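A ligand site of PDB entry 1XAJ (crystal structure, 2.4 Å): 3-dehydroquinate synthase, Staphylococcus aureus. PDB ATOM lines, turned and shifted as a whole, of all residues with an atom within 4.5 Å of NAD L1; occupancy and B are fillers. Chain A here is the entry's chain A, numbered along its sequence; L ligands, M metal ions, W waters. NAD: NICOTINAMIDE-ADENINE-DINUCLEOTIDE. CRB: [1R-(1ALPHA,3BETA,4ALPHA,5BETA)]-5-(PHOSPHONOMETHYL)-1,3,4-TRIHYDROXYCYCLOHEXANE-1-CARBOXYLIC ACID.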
ATOM      1  N   ASP A  39      -0.175 -24.595 -34.872  1.00  0.00           N
ATOM      2  CA  ASP A  39      -0.953 -23.817 -33.922  1.00  0.00           C
ATOM      3  C   ASP A  39      -1.883 -22.894 -34.693  1.00  0.00           C
ATOM      4  O   ASP A  39      -1.513 -22.356 -35.729  1.00  0.00           O
ATOM      5  CB  ASP A  39       0.001 -22.992 -33.055  1.00  0.00           C
ATOM      6  CG  ASP A  39      -0.672 -22.391 -31.861  1.00  0.00           C
ATOM      7  OD1 ASP A  39      -1.763 -21.795 -32.017  1.00  0.00           O
ATOM      8  OD2 ASP A  39      -0.107 -22.505 -30.749  1.00  0.00           O
ATOM      9  N   TYR A  41      -2.923 -19.862 -34.024  1.00  0.00           N
ATOM     10  CA  TYR A  41      -2.357 -18.521 -34.134  1.00  0.00           C
ATOM     11  C   TYR A  41      -1.148 -18.504 -35.028  1.00  0.00           C
ATOM     12  O   TYR A  41      -0.995 -17.605 -35.861  1.00  0.00           O
ATOM     13  CB  TYR A  41      -1.987 -17.961 -32.771  1.00  0.00           C
ATOM     14  CG  TYR A  41      -3.181 -17.652 -31.902  1.00  0.00           C
ATOM     15  CD1 TYR A  41      -3.040 -17.467 -30.528  1.00  0.00           C
ATOM     16  CD2 TYR A  41      -4.463 -17.566 -32.455  1.00  0.00           C
ATOM     17  CE1 TYR A  41      -4.140 -17.204 -29.725  1.00  0.00           C
ATOM     18  CE2 TYR A  41      -5.571 -17.303 -31.658  1.00  0.00           C
ATOM     19  CZ  TYR A  41      -5.403 -17.127 -30.285  1.00  0.00           C
ATOM     20  OH  TYR A  41      -6.491 -16.873 -29.496  1.00  0.00           O
ATOM     21  N   VAL A  42      -0.269 -19.493 -34.864  1.00  0.00           N
ATOM     22  CA  VAL A  42       0.936 -19.573 -35.677  1.00  0.00           C
ATOM     23  C   VAL A  42       0.558 -19.626 -37.153  1.00  0.00           C
ATOM     24  O   VAL A  42       1.211 -19.005 -37.991  1.00  0.00           O
ATOM     25  CB  VAL A  42       1.788 -20.825 -35.336  1.00  0.00           C
ATOM     26  CG1 VAL A  42       3.063 -20.819 -36.165  1.00  0.00           C
ATOM     27  CG2 VAL A  42       2.128 -20.827 -33.853  1.00  0.00           C
ATOM     28  N   TYR A  45      -0.125 -16.270 -38.421  1.00  0.00           N
ATOM     29  CA  TYR A  45       1.168 -15.610 -38.551  1.00  0.00           C
ATOM     30  C   TYR A  45       2.000 -16.022 -39.758  1.00  0.00           C
ATOM     31  O   TYR A  45       2.421 -15.173 -40.538  1.00  0.00           O
ATOM     32  CB  TYR A  45       1.999 -15.866 -37.292  1.00  0.00           C
ATOM     33  CG  TYR A  45       1.803 -14.871 -36.165  1.00  0.00           C
ATOM     34  CD1 TYR A  45       2.257 -13.557 -36.277  1.00  0.00           C
ATOM     35  CD2 TYR A  45       1.215 -15.271 -34.965  1.00  0.00           C
ATOM     36  CE1 TYR A  45       2.138 -12.667 -35.204  1.00  0.00           C
ATOM     37  CE2 TYR A  45       1.102 -14.385 -33.900  1.00  0.00           C
ATOM     38  CZ  TYR A  45       1.557 -13.090 -34.027  1.00  0.00           C
ATOM     39  OH  TYR A  45       1.472 -12.238 -32.944  1.00  0.00           O
ATOM     40  N   PHE A  46       2.249 -17.319 -39.896  1.00  0.00           N
ATOM     41  CA  PHE A  46       3.076 -17.814 -40.990  1.00  0.00           C
ATOM     42  C   PHE A  46       2.376 -18.766 -41.954  1.00  0.00           C
ATOM     43  O   PHE A  46       2.975 -19.741 -42.410  1.00  0.00           O
ATOM     44  CB  PHE A  46       4.324 -18.510 -40.422  1.00  0.00           C
ATOM     45  CG  PHE A  46       5.030 -17.728 -39.333  1.00  0.00           C
ATOM     46  CD1 PHE A  46       4.602 -17.810 -38.015  1.00  0.00           C
ATOM     47  CD2 PHE A  46       6.092 -16.873 -39.647  1.00  0.00           C
ATOM     48  CE1 PHE A  46       5.228 -17.059 -37.015  1.00  0.00           C
ATOM     49  CE2 PHE A  46       6.714 -16.115 -38.658  1.00  0.00           C
ATOM     50  CZ  PHE A  46       6.283 -16.205 -37.336  1.00  0.00           C
ATOM     51  N   GLY A  67      -2.034 -22.768 -28.623  1.00  0.00           N
ATOM     52  CA  GLY A  67      -1.292 -23.094 -27.420  1.00  0.00           C
ATOM     53  C   GLY A  67      -1.725 -24.246 -26.541  1.00  0.00           C
ATOM     54  O   GLY A  67      -2.010 -25.334 -27.012  1.00  0.00           O
ATOM     55  N   GLU A  68      -1.744 -23.968 -25.234  1.00  0.00           N
ATOM     56  CA  GLU A  68      -2.087 -24.937 -24.199  1.00  0.00           C
ATOM     57  C   GLU A  68      -3.479 -25.554 -24.304  1.00  0.00           C
ATOM     58  O   GLU A  68      -3.833 -26.470 -23.554  1.00  0.00           O
ATOM     59  CB  GLU A  68      -1.946 -24.254 -22.834  1.00  0.00           C
ATOM     60  CG  GLU A  68      -1.900 -25.203 -21.648  1.00  0.00           C
ATOM     61  CD  GLU A  68      -0.574 -25.922 -21.518  1.00  0.00           C
ATOM     62  OE1 GLU A  68      -0.386 -26.664 -20.536  1.00  0.00           O
ATOM     63  OE2 GLU A  68       0.281 -25.733 -22.401  1.00  0.00           O
ATOM     64  N   LYS A  71      -3.597 -29.447 -25.868  1.00  0.00           N
ATOM     65  CA  LYS A  71      -3.168 -30.592 -25.066  1.00  0.00           C
ATOM     66  C   LYS A  71      -4.236 -31.250 -24.166  1.00  0.00           C
ATOM     67  O   LYS A  71      -4.149 -31.176 -22.938  1.00  0.00           O
ATOM     68  CB  LYS A  71      -1.955 -30.182 -24.223  1.00  0.00           C
ATOM     69  CG  LYS A  71      -0.764 -29.763 -25.073  1.00  0.00           C
ATOM     70  CD  LYS A  71       0.359 -29.155 -24.252  1.00  0.00           C
ATOM     71  CE  LYS A  71       0.992 -30.133 -23.291  1.00  0.00           C
ATOM     72  NZ  LYS A  71       2.061 -29.484 -22.486  1.00  0.00           N
ATOM     73  N   GLY A  99       4.703 -23.751 -30.808  1.00  0.00           N
ATOM     74  CA  GLY A  99       5.445 -23.737 -29.563  1.00  0.00           C
ATOM     75  C   GLY A  99       5.492 -25.066 -28.822  1.00  0.00           C
ATOM     76  O   GLY A  99       5.197 -26.124 -29.381  1.00  0.00           O
ATOM     77  N   GLY A 100       5.857 -25.006 -27.556  1.00  0.00           N
ATOM     78  CA  GLY A 100       5.959 -26.208 -26.754  1.00  0.00           C
ATOM     79  C   GLY A 100       4.678 -27.000 -26.655  1.00  0.00           C
ATOM     80  O   GLY A 100       4.696 -28.219 -26.717  1.00  0.00           O
ATOM     81  N   ALA A 101       3.557 -26.299 -26.508  1.00  0.00           N
ATOM     82  CA  ALA A 101       2.268 -26.969 -26.397  1.00  0.00           C
ATOM     83  C   ALA A 101       1.992 -27.770 -27.659  1.00  0.00           C
ATOM     84  O   ALA A 101       1.561 -28.926 -27.610  1.00  0.00           O
ATOM     85  CB  ALA A 101       1.162 -25.953 -26.177  1.00  0.00           C
ATOM     86  N   THR A 102       2.238 -27.140 -28.791  1.00  0.00           N
ATOM     87  CA  THR A 102       2.012 -27.744 -30.090  1.00  0.00           C
ATOM     88  C   THR A 102       2.953 -28.906 -30.377  1.00  0.00           C
ATOM     89  O   THR A 102       2.542 -29.904 -30.973  1.00  0.00           O
ATOM     90  CB  THR A 102       2.134 -26.687 -31.210  1.00  0.00           C
ATOM     91  OG1 THR A 102       0.924 -25.909 -31.268  1.00  0.00           O
ATOM     92  CG2 THR A 102       2.379 -27.340 -32.552  1.00  0.00           C
ATOM     93  N   ASP A 104       4.598 -30.697 -27.997  1.00  0.00           N
ATOM     94  CA  ASP A 104       4.317 -31.724 -27.003  1.00  0.00           C
ATOM     95  C   ASP A 104       3.190 -32.559 -27.533  1.00  0.00           C
ATOM     96  O   ASP A 104       3.294 -33.782 -27.624  1.00  0.00           O
ATOM     97  CB  ASP A 104       3.863 -31.102 -25.683  1.00  0.00           C
ATOM     98  CG  ASP A 104       5.019 -30.716 -24.781  1.00  0.00           C
ATOM     99  OD1 ASP A 104       4.742 -30.394 -23.605  1.00  0.00           O
ATOM    100  OD2 ASP A 104       6.192 -30.733 -25.234  1.00  0.00           O
ATOM    101  N   THR A 124       8.695 -22.644 -32.822  1.00  0.00           N
ATOM    102  CA  THR A 124       8.533 -21.251 -33.229  1.00  0.00           C
ATOM    103  C   THR A 124       8.569 -20.251 -32.074  1.00  0.00           C
ATOM    104  O   THR A 124       8.425 -19.046 -32.288  1.00  0.00           O
ATOM    105  CB  THR A 124       7.202 -21.055 -33.991  1.00  0.00           C
ATOM    106  OG1 THR A 124       6.124 -21.536 -33.180  1.00  0.00           O
ATOM    107  CG2 THR A 124       7.223 -21.818 -35.311  1.00  0.00           C
ATOM    108  N   THR A 125       8.770 -20.733 -30.846  1.00  0.00           N
ATOM    109  CA  THR A 125       8.834 -19.861 -29.680  1.00  0.00           C
ATOM    110  C   THR A 125      10.191 -19.956 -29.028  1.00  0.00           C
ATOM    111  O   THR A 125      10.984 -20.843 -29.352  1.00  0.00           O
ATOM    112  CB  THR A 125       7.797 -20.241 -28.608  1.00  0.00           C
ATOM    113  OG1 THR A 125       8.184 -21.477 -28.002  1.00  0.00           O
ATOM    114  CG2 THR A 125       6.412 -20.372 -29.199  1.00  0.00           C
ATOM    115  N   LEU A 127      10.682 -20.336 -25.616  1.00  0.00           N
ATOM    116  CA  LEU A 127      10.588 -21.403 -24.644  1.00  0.00           C
ATOM    117  C   LEU A 127      10.734 -22.747 -25.357  1.00  0.00           C
ATOM    118  O   LEU A 127      11.125 -23.746 -24.751  1.00  0.00           O
ATOM    119  CB  LEU A 127       9.250 -21.313 -23.891  1.00  0.00           C
ATOM    120  CG  LEU A 127       9.079 -22.020 -22.538  1.00  0.00           C
ATOM    121  CD1 LEU A 127       7.906 -21.423 -21.794  1.00  0.00           C
ATOM    122  CD2 LEU A 127       8.883 -23.513 -22.751  1.00  0.00           C
ATOM    123  N   ALA A 128      10.446 -22.767 -26.661  1.00  0.00           N
ATOM    124  CA  ALA A 128      10.506 -23.990 -27.458  1.00  0.00           C
ATOM    125  C   ALA A 128      11.913 -24.478 -27.782  1.00  0.00           C
ATOM    126  O   ALA A 128      12.074 -25.476 -28.474  1.00  0.00           O
ATOM    127  CB  ALA A 128       9.729 -23.820 -28.744  1.00  0.00           C
ATOM    128  N   ASP A 130      13.721 -25.360 -25.504  1.00  0.00           N
ATOM    129  CA  ASP A 130      13.772 -26.349 -24.449  1.00  0.00           C
ATOM    130  C   ASP A 130      12.848 -27.486 -24.847  1.00  0.00           C
ATOM    131  O   ASP A 130      13.281 -28.596 -25.109  1.00  0.00           O
ATOM    132  CB  ASP A 130      13.309 -25.705 -23.137  1.00  0.00           C
ATOM    133  CG  ASP A 130      12.975 -26.724 -22.059  1.00  0.00           C
ATOM    134  OD1 ASP A 130      13.638 -27.776 -21.989  1.00  0.00           O
ATOM    135  OD2 ASP A 130      12.044 -26.461 -21.277  1.00  0.00           O
ATOM    136  N   SER A 131      11.557 -27.174 -24.926  1.00  0.00           N
ATOM    137  CA  SER A 131      10.529 -28.142 -25.292  1.00  0.00           C
ATOM    138  C   SER A 131      10.793 -28.991 -26.554  1.00  0.00           C
ATOM    139  O   SER A 131      10.372 -30.145 -26.617  1.00  0.00           O
ATOM    140  CB  SER A 131       9.179 -27.424 -25.441  1.00  0.00           C
ATOM    141  OG  SER A 131       9.238 -26.360 -26.367  1.00  0.00           O
ATOM    142  N   VAL A 133      13.651 -30.084 -27.618  1.00  0.00           N
ATOM    143  CA  VAL A 133      14.745 -31.025 -27.394  1.00  0.00           C
ATOM    144  C   VAL A 133      14.424 -31.895 -26.187  1.00  0.00           C
ATOM    145  O   VAL A 133      13.616 -31.525 -25.347  1.00  0.00           O
ATOM    146  CB  VAL A 133      16.074 -30.246 -27.130  1.00  0.00           C
ATOM    147  CG1 VAL A 133      17.154 -31.200 -26.627  1.00  0.00           C
ATOM    148  CG2 VAL A 133      16.532 -29.551 -28.410  1.00  0.00           C
ATOM    149  N   LYS A 136      10.535 -35.293 -24.791  1.00  0.00           N
ATOM    150  CA  LYS A 136       9.371 -35.427 -23.926  1.00  0.00           C
ATOM    151  C   LYS A 136       8.172 -34.843 -24.656  1.00  0.00           C
ATOM    152  O   LYS A 136       8.252 -33.750 -25.241  1.00  0.00           O
ATOM    153  CB  LYS A 136       9.557 -34.688 -22.607  1.00  0.00           C
ATOM    154  CG  LYS A 136      10.244 -35.477 -21.525  1.00  0.00           C
ATOM    155  CD  LYS A 136      10.138 -34.752 -20.191  1.00  0.00           C
ATOM    156  CE  LYS A 136      10.937 -35.443 -19.100  1.00  0.00           C
ATOM    157  NZ  LYS A 136      10.995 -34.598 -17.874  1.00  0.00           N
ATOM    158  N   VAL A 137       7.058 -35.559 -24.633  1.00  0.00           N
ATOM    159  CA  VAL A 137       5.855 -35.119 -25.310  1.00  0.00           C
ATOM    160  C   VAL A 137       4.677 -35.588 -24.487  1.00  0.00           C
ATOM    161  O   VAL A 137       4.820 -36.506 -23.687  1.00  0.00           O
ATOM    162  CB  VAL A 137       5.756 -35.750 -26.735  1.00  0.00           C
ATOM    163  CG1 VAL A 137       6.988 -35.394 -27.550  1.00  0.00           C
ATOM    164  CG2 VAL A 137       5.609 -37.269 -26.635  1.00  0.00           C
ATOM    165  N   LYS A 145      -0.508 -30.703 -15.162  1.00  0.00           N
ATOM    166  CA  LYS A 145       0.374 -30.512 -16.292  1.00  0.00           C
ATOM    167  C   LYS A 145       1.218 -31.722 -16.643  1.00  0.00           C
ATOM    168  O   LYS A 145       1.989 -32.217 -15.832  1.00  0.00           O
ATOM    169  CB  LYS A 145       1.333 -29.339 -16.039  1.00  0.00           C
ATOM    170  CG  LYS A 145       0.808 -27.970 -16.469  1.00  0.00           C
ATOM    171  CD  LYS A 145       0.597 -27.902 -17.978  1.00  0.00           C
ATOM    172  CE  LYS A 145       1.879 -28.179 -18.750  1.00  0.00           C
ATOM    173  NZ  LYS A 145       2.958 -27.203 -18.435  1.00  0.00           N
ATOM    174  N   ASN A 146       1.049 -32.193 -17.868  1.00  0.00           N
ATOM    175  CA  ASN A 146       1.816 -33.315 -18.391  1.00  0.00           C
ATOM    176  C   ASN A 146       1.709 -34.663 -17.663  1.00  0.00           C
ATOM    177  O   ASN A 146       2.734 -35.258 -17.326  1.00  0.00           O
ATOM    178  CB  ASN A 146       3.306 -32.916 -18.452  1.00  0.00           C
ATOM    179  CG  ASN A 146       3.525 -31.589 -19.159  1.00  0.00           C
ATOM    180  OD1 ASN A 146       2.616 -31.039 -19.768  1.00  0.00           O
ATOM    181  ND2 ASN A 146       4.759 -31.077 -19.084  1.00  0.00           N
ATOM    182  N   PHE A 163      11.570 -17.063 -36.504  1.00  0.00           N
ATOM    183  CA  PHE A 163      10.250 -17.212 -35.909  1.00  0.00           C
ATOM    184  C   PHE A 163      10.012 -16.291 -34.721  1.00  0.00           C
ATOM    185  O   PHE A 163       8.899 -15.817 -34.495  1.00  0.00           O
ATOM    186  CB  PHE A 163      10.025 -18.669 -35.457  1.00  0.00           C
ATOM    187  CG  PHE A 163       9.674 -19.620 -36.573  1.00  0.00           C
ATOM    188  CD1 PHE A 163       8.533 -19.430 -37.333  1.00  0.00           C
ATOM    189  CD2 PHE A 163      10.497 -20.708 -36.848  1.00  0.00           C
ATOM    190  CE1 PHE A 163       8.206 -20.311 -38.358  1.00  0.00           C
ATOM    191  CE2 PHE A 163      10.174 -21.603 -37.876  1.00  0.00           C
ATOM    192  CZ  PHE A 163       9.029 -21.400 -38.633  1.00  0.00           C
ATOM    193  N   THR A 166       8.348 -12.235 -34.040  1.00  0.00           N
ATOM    194  CA  THR A 166       6.943 -11.889 -33.897  1.00  0.00           C
ATOM    195  C   THR A 166       6.322 -12.222 -32.549  1.00  0.00           C
ATOM    196  O   THR A 166       5.110 -12.101 -32.382  1.00  0.00           O
ATOM    197  CB  THR A 166       6.126 -12.569 -35.003  1.00  0.00           C
ATOM    198  OG1 THR A 166       6.347 -13.989 -34.959  1.00  0.00           O
ATOM    199  CG2 THR A 166       6.566 -12.046 -36.370  1.00  0.00           C
ATOM    200  N   LEU A 167       7.140 -12.630 -31.596  1.00  0.00           N
ATOM    201  CA  LEU A 167       6.644 -12.965 -30.276  1.00  0.00           C
ATOM    202  C   LEU A 167       6.397 -11.705 -29.440  1.00  0.00           C
ATOM    203  O   LEU A 167       7.260 -10.828 -29.341  1.00  0.00           O
ATOM    204  CB  LEU A 167       7.646 -13.865 -29.534  1.00  0.00           C
ATOM    205  CG  LEU A 167       7.853 -15.314 -29.973  1.00  0.00           C
ATOM    206  CD1 LEU A 167       9.071 -15.878 -29.285  1.00  0.00           C
ATOM    207  CD2 LEU A 167       6.618 -16.133 -29.637  1.00  0.00           C
ATOM    208  N   PRO A 168       5.195 -11.581 -28.848  1.00  0.00           N
ATOM    209  CA  PRO A 168       4.914 -10.409 -28.024  1.00  0.00           C
ATOM    210  C   PRO A 168       5.837 -10.525 -26.801  1.00  0.00           C
ATOM    211  O   PRO A 168       6.414 -11.591 -26.570  1.00  0.00           O
ATOM    212  CB  PRO A 168       3.438 -10.602 -27.664  1.00  0.00           C
ATOM    213  CG  PRO A 168       2.909 -11.427 -28.812  1.00  0.00           C
ATOM    214  CD  PRO A 168       3.999 -12.424 -28.999  1.00  0.00           C
ATOM    215  N   GLN A 171       5.402 -13.501 -24.201  1.00  0.00           N
ATOM    216  CA  GLN A 171       5.980 -14.779 -24.565  1.00  0.00           C
ATOM    217  C   GLN A 171       7.496 -14.733 -24.488  1.00  0.00           C
ATOM    218  O   GLN A 171       8.145 -15.758 -24.271  1.00  0.00           O
ATOM    219  CB  GLN A 171       5.536 -15.188 -25.965  1.00  0.00           C
ATOM    220  CG  GLN A 171       4.039 -15.365 -26.067  1.00  0.00           C
ATOM    221  CD  GLN A 171       3.483 -16.307 -25.008  1.00  0.00           C
ATOM    222  OE1 GLN A 171       2.308 -16.235 -24.656  1.00  0.00           O
ATOM    223  NE2 GLN A 171       4.330 -17.198 -24.508  1.00  0.00           N
ATOM    224  N   LYS A 221      21.066 -28.359 -22.113  1.00  0.00           N
ATOM    225  CA  LYS A 221      20.105 -29.435 -21.870  1.00  0.00           C
ATOM    226  C   LYS A 221      20.502 -30.668 -22.657  1.00  0.00           C
ATOM    227  O   LYS A 221      20.371 -31.792 -22.167  1.00  0.00           O
ATOM    228  CB  LYS A 221      18.697 -28.995 -22.303  1.00  0.00           C
ATOM    229  CG  LYS A 221      17.628 -30.075 -22.133  1.00  0.00           C
ATOM    230  CD  LYS A 221      16.300 -29.644 -22.731  1.00  0.00           C
ATOM    231  CE  LYS A 221      15.239 -30.683 -22.494  1.00  0.00           C
ATOM    232  NZ  LYS A 221      13.907 -30.274 -23.020  1.00  0.00           N
ATOM    233  N   HIS A 256       3.536 -20.393 -18.781  1.00  0.00           N
ATOM    234  CA  HIS A 256       4.402 -21.385 -18.195  1.00  0.00           C
ATOM    235  C   HIS A 256       5.669 -20.724 -17.661  1.00  0.00           C
ATOM    236  O   HIS A 256       5.968 -20.801 -16.458  1.00  0.00           O
ATOM    237  CB  HIS A 256       4.740 -22.433 -19.253  1.00  0.00           C
ATOM    238  CG  HIS A 256       5.616 -23.524 -18.751  1.00  0.00           C
ATOM    239  ND1 HIS A 256       5.379 -24.186 -17.561  1.00  0.00           N
ATOM    240  CD2 HIS A 256       6.744 -24.080 -19.263  1.00  0.00           C
ATOM    241  CE1 HIS A 256       6.318 -25.099 -17.370  1.00  0.00           C
ATOM    242  NE2 HIS A 256       7.149 -25.046 -18.386  1.00  0.00           N
HETATM  243  PA  NAD L   1       2.662 -22.386 -26.741  1.00  0.00           P
HETATM  244  O1A NAD L   1       2.325 -23.290 -27.848  1.00  0.00           O
HETATM  245  O2A NAD L   1       1.505 -22.252 -25.835  1.00  0.00           O
HETATM  246  O5B NAD L   1       3.077 -20.936 -27.339  1.00  0.00           O
HETATM  247  C5B NAD L   1       2.769 -19.723 -26.565  1.00  0.00           C
HETATM  248  C4B NAD L   1       1.927 -18.791 -27.433  1.00  0.00           C
HETATM  249  O4B NAD L   1       2.662 -18.181 -28.537  1.00  0.00           O
HETATM  250  C3B NAD L   1       0.703 -19.383 -28.112  1.00  0.00           C
HETATM  251  O3B NAD L   1      -0.469 -18.557 -27.948  1.00  0.00           O
HETATM  252  C2B NAD L   1       1.060 -19.492 -29.610  1.00  0.00           C
HETATM  253  O2B NAD L   1      -0.085 -19.429 -30.447  1.00  0.00           O
HETATM  254  C1B NAD L   1       1.968 -18.328 -29.796  1.00  0.00           C
HETATM  255  N9A NAD L   1       3.104 -18.405 -30.715  1.00  0.00           N
HETATM  256  C8A NAD L   1       3.778 -19.586 -31.081  1.00  0.00           C
HETATM  257  N7A NAD L   1       4.623 -19.345 -32.054  1.00  0.00           N
HETATM  258  C5A NAD L   1       4.692 -17.963 -32.153  1.00  0.00           C
HETATM  259  C6A NAD L   1       5.544 -17.086 -32.885  1.00  0.00           C
HETATM  260  N6A NAD L   1       6.636 -17.469 -33.535  1.00  0.00           N
HETATM  261  N1A NAD L   1       5.184 -15.741 -32.904  1.00  0.00           N
HETATM  262  C2A NAD L   1       4.147 -15.318 -32.087  1.00  0.00           C
HETATM  263  N3A NAD L   1       3.369 -16.033 -31.258  1.00  0.00           N
HETATM  264  C4A NAD L   1       3.706 -17.388 -31.370  1.00  0.00           C
HETATM  265  O3  NAD L   1       3.892 -23.003 -25.916  1.00  0.00           O
HETATM  266  PN  NAD L   1       5.244 -22.448 -25.266  1.00  0.00           P
HETATM  267  O1N NAD L   1       6.256 -22.231 -26.288  1.00  0.00           O
HETATM  268  O2N NAD L   1       4.985 -21.157 -24.565  1.00  0.00           O
HETATM  269  O5D NAD L   1       5.753 -23.536 -24.199  1.00  0.00           O
HETATM  270  C5D NAD L   1       4.943 -23.947 -23.105  1.00  0.00           C
HETATM  271  C4D NAD L   1       4.484 -25.376 -23.363  1.00  0.00           C
HETATM  272  O4D NAD L   1       5.670 -26.203 -23.545  1.00  0.00           O
HETATM  273  C3D NAD L   1       3.711 -26.000 -22.193  1.00  0.00           C
HETATM  274  O3D NAD L   1       2.647 -26.740 -22.751  1.00  0.00           O
HETATM  275  C2D NAD L   1       4.757 -26.843 -21.498  1.00  0.00           C
HETATM  276  O2D NAD L   1       4.200 -27.883 -20.670  1.00  0.00           O
HETATM  277  C1D NAD L   1       5.581 -27.365 -22.650  1.00  0.00           C
HETATM  278  N1N NAD L   1       6.976 -27.704 -22.375  1.00  0.00           N
HETATM  279  C2N NAD L   1       7.305 -28.959 -22.861  1.00  0.00           C
HETATM  280  C3N NAD L   1       8.591 -29.455 -22.641  1.00  0.00           C
HETATM  281  C7N NAD L   1       8.965 -30.934 -22.948  1.00  0.00           C
HETATM  282  O7N NAD L   1       8.111 -31.707 -23.379  1.00  0.00           O
HETATM  283  N7N NAD L   1      10.250 -31.334 -22.721  1.00  0.00           N
HETATM  284  C4N NAD L   1       9.655 -28.635 -22.109  1.00  0.00           C
HETATM  285  C5N NAD L   1       9.222 -27.348 -21.689  1.00  0.00           C
HETATM  286  C6N NAD L   1       7.933 -26.865 -21.693  1.00  0.00           C
HETATM  287  C1  CRB L   2      12.822 -31.979 -19.413  1.00  0.00           C
HETATM  288  O11 CRB L   2      13.220 -33.073 -18.837  1.00  0.00           O
HETATM  289  O12 CRB L   2      13.025 -31.678 -20.615  1.00  0.00           O
HETATM  290  C2  CRB L   2      12.039 -30.988 -18.497  1.00  0.00           C
HETATM  291  O2  CRB L   2      12.371 -31.251 -17.136  1.00  0.00           O
HETATM  292  C3  CRB L   2      12.314 -29.486 -18.775  1.00  0.00           C
HETATM  293  C4  CRB L   2      11.242 -28.529 -18.201  1.00  0.00           C
HETATM  294  O4  CRB L   2      11.426 -27.172 -18.721  1.00  0.00           O
HETATM  295  C5  CRB L   2       9.795 -29.026 -18.541  1.00  0.00           C
HETATM  296  O5  CRB L   2       8.868 -28.147 -17.997  1.00  0.00           O
HETATM  297  C6  CRB L   2       9.627 -30.476 -18.016  1.00  0.00           C
HETATM  298  C7  CRB L   2       8.215 -31.056 -18.148  1.00  0.00           C
HETATM  299  C8  CRB L   2      10.535 -31.369 -18.745  1.00  0.00           C
HETATM  300  P1  CRB L   2       7.665 -32.211 -16.860  1.00  0.00           P
HETATM  301  O91 CRB L   2       8.057 -31.644 -15.542  1.00  0.00           O
HETATM  302  O92 CRB L   2       8.423 -33.480 -17.242  1.00  0.00           O
HETATM  303  O93 CRB L   2       6.103 -32.291 -17.086  1.00  0.00           O
HETATM  304 ZN    ZN M   1       9.446 -25.566 -18.736  1.00  0.00          ZN
HETATM  305  O   HOH W   1       6.284 -19.011 -25.994  1.00  0.00           O
HETATM  306  O   HOH W   2       6.015 -27.923 -18.610  1.00  0.00           O
HETATM  307  O   HOH W   3       3.872 -19.752 -22.480  1.00  0.00           O
HETATM  308  O   HOH W   4      12.244 -32.752 -23.752  1.00  0.00           O
HETATM  309  O   HOH W   5      -2.576 -19.930 -26.471  1.00  0.00           O
HETATM  310  O   HOH W   6       1.913 -23.052 -23.195  1.00  0.00           O
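Water W2 lies within hydrogen-bond range of O2D of NAD L1 (2.7 Å), O5 of CRB L2 (2.9 Å), NZ of Lys 145 (3.1 Å) and ND2 of Asn 146 (3.4 Å).
Water W3 bridges O2N of NAD L1 and NE2 of Gln 171.
Water W6 lies within hydrogen-bond range of O2A of NAD L1 (2.8 Å) and OE2 of Glu 68 (3.2 Å).
Water W1 lies within hydrogen-bond range of an oxygen (O2N) of NAD L1 and the side-chain amide nitrogen (NE2) of Gln 171.
The side-chain carboxylate of Asp 104 lies close to an oxygen (O7N) of NAD L1, at 2.8 Å.
The backbone carbonyl oxygen of Lys 136 lies close to an oxygen (O7N) of NAD L1.
Residues that only touch NAD L1: Tyr 41 (3.3 Å), Val 42 (3.4 Å), Tyr 45 (3.7 Å), Phe 46 (3.8 Å), Gly 67 (3.3 Å), Gly 99 (3.6 Å), Thr 102 (3.96 Å), Leu 127 (3.4 Å), Asp 130 (3.0 Å), Ser 131 (3.3 Å), Asn 146 (3.6 Å), Leu 167 (3.6 Å), Gln 171 (3.6 Å), Lys 221 (3.8 Å) and His 256 (3.9 Å).
Within 4 Å of NAD L1: Asp 39, Tyr 41, Val 42, Tyr 45, Phe 46, Gly 67, Glu 68, Lys 71, Gly 99, Gly 100, Ala 101, Thr 102, Asp 104, Thr 124, Thr 125, Leu 127, Asp 130, Ser 131, Lys 136, Lys 145, Asn 146, Phe 163, Thr 166, Leu 167, Gln 171, Lys 221 and His 256.
The side-chain amino group (NZ) of Lys 71 is in salt-bridge range of the side-chain carboxylate (OD1) of Asp 104 (3.0 Å).
The side-chain amino group of Lys 145 is in salt-bridge range of the side-chain carboxylate of Glu 68 (3.99 Å).
The side-chain carboxylate (OD1) of Asp 130 lies within salt-bridge range of the side-chain amino group (NZ) of Lys 221 (2.7 Å).
OD1 of Asp 39 sits at hydrogen-bond distance from N of Tyr 41 (3.0 Å).
O of Phe 163 is in hydrogen-bond range of OG1 of Thr 166 (3.2 Å).
OG1 of Thr 125 lies close to N of Ala 128.
The side-chain amino group (NZ) of Lys 221 is in hydrogen-bond range of the backbone carbonyl oxygen (O) of Val 133, at 2.7 Å.
The side-chain amide oxygen of Asn 146 lies within hydrogen-bond range of the side-chain amino group of Lys 71.
N of Ala 101 sits at hydrogen-bond distance from O3 of NAD L1, at 3.4 Å.
N of Gly 100 lies within hydrogen-bond range of O1N of NAD L1 (3.1 Å).
OE2 of Glu 68 is in hydrogen-bond range of O3D of NAD L1, 2.6 Å away.
The backbone carbonyl oxygen (O) of Thr 124 lies within hydrogen-bond range of a nitrogen (N6A) of NAD L1.
The backbone carbonyl oxygen (O) of Phe 163 sits at hydrogen-bond distance from a nitrogen (N6A) of NAD L1 (3.0 Å).
A nitrogen (N7A) of NAD L1 lies within hydrogen-bond range of the side-chain hydroxyl (OG1) of Thr 124, at 2.9 Å.
The side-chain amino group of Lys 145 lies within hydrogen-bond range of an oxygen (O2D) of NAD L1 (2.6 Å).
OG1 of Thr 166 lies within hydrogen-bond range of N1A of NAD L1 (2.9 Å).
NZ of Lys 136 lies within salt-bridge range of O11 of CRB L2, 2.9 Å away.
The side-chain amino group of Lys 221 lies within salt-bridge range of an oxygen (O12) of CRB L2 (2.9 Å).
An oxygen (O2B) of NAD L1 lies within hydrogen-bond range of the side-chain carboxylate of Asp 39, at 3.1 Å.
OG1 of Thr 125 is in hydrogen-bond range of O1N of NAD L1, at 2.7 Å.
An oxygen (O93) of CRB L2 sits at hydrogen-bond distance from the side-chain amide nitrogen (ND2) of Asn 146 (2.7 Å).
O3D of NAD L1 lies within hydrogen-bond range of NZ of Lys 71.
An oxygen (O4) of CRB L2 lies close to the side-chain carboxylate of Asp 130, at 2.7 Å.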
